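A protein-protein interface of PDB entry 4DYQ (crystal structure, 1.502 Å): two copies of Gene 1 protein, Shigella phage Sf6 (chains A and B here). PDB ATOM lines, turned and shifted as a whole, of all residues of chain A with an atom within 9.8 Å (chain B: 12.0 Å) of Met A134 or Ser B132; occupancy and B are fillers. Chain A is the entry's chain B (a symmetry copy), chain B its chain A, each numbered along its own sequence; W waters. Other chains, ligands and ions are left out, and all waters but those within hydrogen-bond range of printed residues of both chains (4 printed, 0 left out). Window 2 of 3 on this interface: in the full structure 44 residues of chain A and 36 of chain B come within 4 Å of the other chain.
Hydrophobic or aromatic side chains of chain A within 4 Å of the printed part of chain B: Met A134 and Phe A138. Along chain A the printed residues that touch a printed residue of chain B span positions 131 to 138.
Among the printed residues, merely in contact across the chains: Phe A138 with Ser B132, Thr A131 with Ile B129, Met A134 with Glu B130, Ser A132 with Glu B130, Phe A138 with Glu B130, Pro A133 with Glu B130 and Ser A132 with Thr B131.
Water W3 lies within hydrogen-bond range of the side-chain hydroxyl of Ser A132 (2.6 Å), the side-chain amide oxygen of Gln B128 (2.8 Å) and the backbone carbonyl oxygen of Ile B129 (3.2 Å). Water W4 lies within hydrogen-bond range of the backbone carbonyl oxygen (O) of Ser A132, the backbone carbonyl oxygen (O) of Thr B131 and the backbone NH (N) of Met A134. Water W2 lies within hydrogen-bond range of OE1 of Glu B130 (2.8 Å), OG1 of Thr A136 (2.8 Å) and OG of Ser A135 (3.4 Å). Water W1 bridges the side-chain carboxylate of Glu B130 (2.9 Å) and the side-chain hydroxyl of Ser A135 (3.5 Å).
Ser A132 touches Thr B131, but with the chains exchanged Thr A131 does not touch Ser B132 (9.2 Å). 2 positions are printed for both chains. Of the 10 pairs that touch across the chains among the printed residues, none has its exchanged pair printed and touching as well.
Printed residues of chain B within 4 Å of Met A134: Glu B130 and Ser B132. Ser B132 touches two residues of chain A. Of chain B, only Ile B129 (3.0 Å), Glu B130 (3.4 Å) and Thr B131 (3.9 Å) come within 4 Å of Ser A132. Of chain B, only Glu B130 (3.5 Å) comes within 4 Å of Pro A133. Ser A135 touches just one residue of chain B: Glu B130 (2.8 Å). Thr A136 touches none of the printed residues of chain B. Phe A138 touches just these residues of chain B: Glu B130 (3.5 Å) and Ser B132 (3.0 Å). No residue of chain B comes within 4 Å of Gly A139. Of the printed residues of chain A, Ile B129 touches Thr A131 (3.3 Å) and Ser A132 (3.0 Å). Of the printed residues of chain B, Thr A131 touches Ile B129. The nearest residue of chain A that does not touch Ser B132 is Gly A139 (4.4 Å).
N of Ser A132 is in hydrogen-bond range of O of Ile B129, 3.0 Å away. OG of Ser A135 lies within hydrogen-bond range of OE2 of Glu B130 (2.8 Å). The side-chain hydroxyl (OG) of Ser B132 lies close to the side-chain sulfur (SD) of Met A134, at 3.2 Å.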
ATOM      1  N   THR A 131      -5.806 -18.952  20.515  1.00  0.00           N
ATOM      2  CA  THR A 131      -4.382 -18.713  20.677  1.00  0.00           C
ATOM      3  C   THR A 131      -3.601 -19.945  20.243  1.00  0.00           C
ATOM      4  O   THR A 131      -4.048 -21.076  20.423  1.00  0.00           O
ATOM      5  CB  THR A 131      -4.034 -18.360  22.133  1.00  0.00           C
ATOM      6  OG1 THR A 131      -4.479 -19.408  23.000  1.00  0.00           O
ATOM      7  CG2 THR A 131      -4.693 -17.045  22.537  1.00  0.00           C
ATOM      8  N   SER A 132      -2.433 -19.713  19.656  1.00  0.00           N
ATOM      9  CA  SER A 132      -1.596 -20.789  19.140  1.00  0.00           C
ATOM     10  C   SER A 132      -0.136 -20.475  19.400  1.00  0.00           C
ATOM     11  O   SER A 132       0.230 -19.315  19.588  1.00  0.00           O
ATOM     12  CB  SER A 132      -1.806 -20.953  17.635  1.00  0.00           C
ATOM     13  OG  SER A 132      -3.147 -21.292  17.338  1.00  0.00           O
ATOM     14  N   PRO A 133       0.706 -21.516  19.403  1.00  0.00           N
ATOM     15  CA  PRO A 133       2.148 -21.311  19.555  1.00  0.00           C
ATOM     16  C   PRO A 133       2.656 -20.431  18.428  1.00  0.00           C
ATOM     17  O   PRO A 133       2.088 -20.452  17.333  1.00  0.00           O
ATOM     18  CB  PRO A 133       2.724 -22.727  19.436  1.00  0.00           C
ATOM     19  CG  PRO A 133       1.569 -23.656  19.652  1.00  0.00           C
ATOM     20  CD  PRO A 133       0.362 -22.925  19.164  1.00  0.00           C
ATOM     21  N   MET A 134       3.706 -19.661  18.677  1.00  0.00           N
ATOM     22  CA  MET A 134       4.247 -18.829  17.617  1.00  0.00           C
ATOM     23  C   MET A 134       4.697 -19.734  16.479  1.00  0.00           C
ATOM     24  O   MET A 134       5.239 -20.825  16.704  1.00  0.00           O
ATOM     25  CB  MET A 134       5.378 -17.927  18.120  1.00  0.00           C
ATOM     26  CG  MET A 134       6.461 -18.620  18.891  1.00  0.00           C
ATOM     27  SD  MET A 134       7.414 -17.400  19.810  1.00  0.00           S
ATOM     28  CE  MET A 134       7.876 -16.251  18.512  1.00  0.00           C
ATOM     29  N   SER A 135       4.453 -19.287  15.253  1.00  0.00           N
ATOM     30  CA  SER A 135       4.798 -20.068  14.074  1.00  0.00           C
ATOM     31  C   SER A 135       5.923 -19.412  13.277  1.00  0.00           C
ATOM     32  O   SER A 135       6.400 -19.976  12.296  1.00  0.00           O
ATOM     33  CB  SER A 135       3.565 -20.262  13.193  1.00  0.00           C
ATOM     34  OG  SER A 135       3.130 -19.027  12.668  1.00  0.00           O
ATOM     35  N   THR A 136       6.333 -18.216  13.700  1.00  0.00           N
ATOM     36  CA  THR A 136       7.530 -17.562  13.168  1.00  0.00           C
ATOM     37  C   THR A 136       8.294 -16.856  14.291  1.00  0.00           C
ATOM     38  O   THR A 136       7.752 -16.630  15.372  1.00  0.00           O
ATOM     39  CB  THR A 136       7.176 -16.523  12.101  1.00  0.00           C
ATOM     40  OG1 THR A 136       6.420 -15.462  12.700  1.00  0.00           O
ATOM     41  CG2 THR A 136       6.366 -17.156  10.986  1.00  0.00           C
ATOM     42  N   LEU A 137       9.548 -16.497  14.023  1.00  0.00           N
ATOM     43  CA  LEU A 137      10.406 -15.840  15.005  1.00  0.00           C
ATOM     44  C   LEU A 137      10.165 -14.343  15.047  1.00  0.00           C
ATOM     45  O   LEU A 137      10.922 -13.577  14.451  1.00  0.00           O
ATOM     46  CB  LEU A 137      11.872 -16.065  14.648  1.00  0.00           C
ATOM     47  CG  LEU A 137      12.473 -17.403  15.056  1.00  0.00           C
ATOM     48  CD1 LEU A 137      13.771 -17.666  14.291  1.00  0.00           C
ATOM     49  CD2 LEU A 137      12.719 -17.441  16.553  1.00  0.00           C
ATOM     50  N   PHE A 138       9.140 -13.919  15.775  1.00  0.00           N
ATOM     51  CA  PHE A 138       8.780 -12.503  15.798  1.00  0.00           C
ATOM     52  C   PHE A 138       9.127 -11.766  17.090  1.00  0.00           C
ATOM     53  O   PHE A 138       8.868 -10.570  17.214  1.00  0.00           O
ATOM     54  CB  PHE A 138       7.299 -12.313  15.470  1.00  0.00           C
ATOM     55  CG  PHE A 138       6.342 -12.958  16.442  1.00  0.00           C
ATOM     56  CD1 PHE A 138       6.202 -12.479  17.739  1.00  0.00           C
ATOM     57  CD2 PHE A 138       5.503 -13.980  16.023  1.00  0.00           C
ATOM     58  CE1 PHE A 138       5.278 -13.047  18.605  1.00  0.00           C
ATOM     59  CE2 PHE A 138       4.582 -14.543  16.884  1.00  0.00           C
ATOM     60  CZ  PHE A 138       4.458 -14.072  18.170  1.00  0.00           C
ATOM     61  N   GLY A 139       9.714 -12.474  18.045  1.00  0.00           N
ATOM     62  CA  GLY A 139      10.170 -11.861  19.279  1.00  0.00           C
ATOM     63  C   GLY A 139      11.335 -10.912  19.055  1.00  0.00           C
ATOM     64  O   GLY A 139      11.829 -10.761  17.939  1.00  0.00           O
ATOM     65  N   GLN B 128      -7.260 -15.058  15.382  1.00  0.00           N
ATOM     66  CA  GLN B 128      -6.061 -15.862  15.607  1.00  0.00           C
ATOM     67  C   GLN B 128      -4.957 -15.028  16.230  1.00  0.00           C
ATOM     68  O   GLN B 128      -4.549 -14.021  15.664  1.00  0.00           O
ATOM     69  CB  GLN B 128      -5.555 -16.437  14.277  1.00  0.00           C
ATOM     70  CG  GLN B 128      -6.565 -17.334  13.576  1.00  0.00           C
ATOM     71  CD  GLN B 128      -6.868 -18.585  14.365  1.00  0.00           C
ATOM     72  OE1 GLN B 128      -5.961 -19.288  14.807  1.00  0.00           O
ATOM     73  NE2 GLN B 128      -8.145 -18.861  14.558  1.00  0.00           N
ATOM     74  N   ILE B 129      -4.478 -15.453  17.397  1.00  0.00           N
ATOM     75  CA  ILE B 129      -3.409 -14.764  18.103  1.00  0.00           C
ATOM     76  C   ILE B 129      -2.268 -15.736  18.393  1.00  0.00           C
ATOM     77  O   ILE B 129      -2.506 -16.883  18.744  1.00  0.00           O
ATOM     78  CB  ILE B 129      -3.922 -14.180  19.427  1.00  0.00           C
ATOM     79  CG1 ILE B 129      -4.967 -13.098  19.139  1.00  0.00           C
ATOM     80  CG2 ILE B 129      -2.791 -13.583  20.227  1.00  0.00           C
ATOM     81  CD1 ILE B 129      -5.598 -12.486  20.390  1.00  0.00           C
ATOM     82  N   GLU B 130      -1.036 -15.274  18.214  1.00  0.00           N
ATOM     83  CA  GLU B 130       0.147 -16.006  18.651  1.00  0.00           C
ATOM     84  C   GLU B 130       0.862 -15.142  19.673  1.00  0.00           C
ATOM     85  O   GLU B 130       1.043 -13.953  19.443  1.00  0.00           O
ATOM     86  CB  GLU B 130       1.078 -16.280  17.465  1.00  0.00           C
ATOM     87  CG  GLU B 130       0.577 -17.351  16.519  1.00  0.00           C
ATOM     88  CD  GLU B 130       1.450 -17.504  15.289  1.00  0.00           C
ATOM     89  OE1 GLU B 130       2.597 -16.997  15.298  1.00  0.00           O
ATOM     90  OE2 GLU B 130       0.982 -18.136  14.314  1.00  0.00           O
ATOM     91  N   THR B 131       1.283 -15.717  20.795  1.00  0.00           N
ATOM     92  CA  THR B 131       2.033 -14.939  21.777  1.00  0.00           C
ATOM     93  C   THR B 131       3.418 -15.516  22.036  1.00  0.00           C
ATOM     94  O   THR B 131       3.636 -16.720  21.919  1.00  0.00           O
ATOM     95  CB  THR B 131       1.285 -14.844  23.120  1.00  0.00           C
ATOM     96  OG1 THR B 131       1.214 -16.138  23.729  1.00  0.00           O
ATOM     97  CG2 THR B 131      -0.119 -14.315  22.910  1.00  0.00           C
ATOM     98  N   SER B 132       4.365 -14.652  22.383  1.00  0.00           N
ATOM     99  CA  SER B 132       5.691 -15.130  22.759  1.00  0.00           C
ATOM    100  C   SER B 132       5.791 -15.278  24.277  1.00  0.00           C
ATOM    101  O   SER B 132       6.770 -14.880  24.909  1.00  0.00           O
ATOM    102  CB  SER B 132       6.789 -14.214  22.208  1.00  0.00           C
ATOM    103  OG  SER B 132       6.898 -14.350  20.802  1.00  0.00           O
HETATM  104  O   HOH W   1       0.566 -16.855  11.703  1.00  0.00           O
HETATM  105  O   HOH W   2       3.624 -15.645  13.125  1.00  0.00           O
HETATM  106  O   HOH W   3      -3.931 -18.884  16.751  1.00  0.00           O
HETATM  107  O   HOH W   4       2.044 -18.828  21.404  1.00  0.00           O
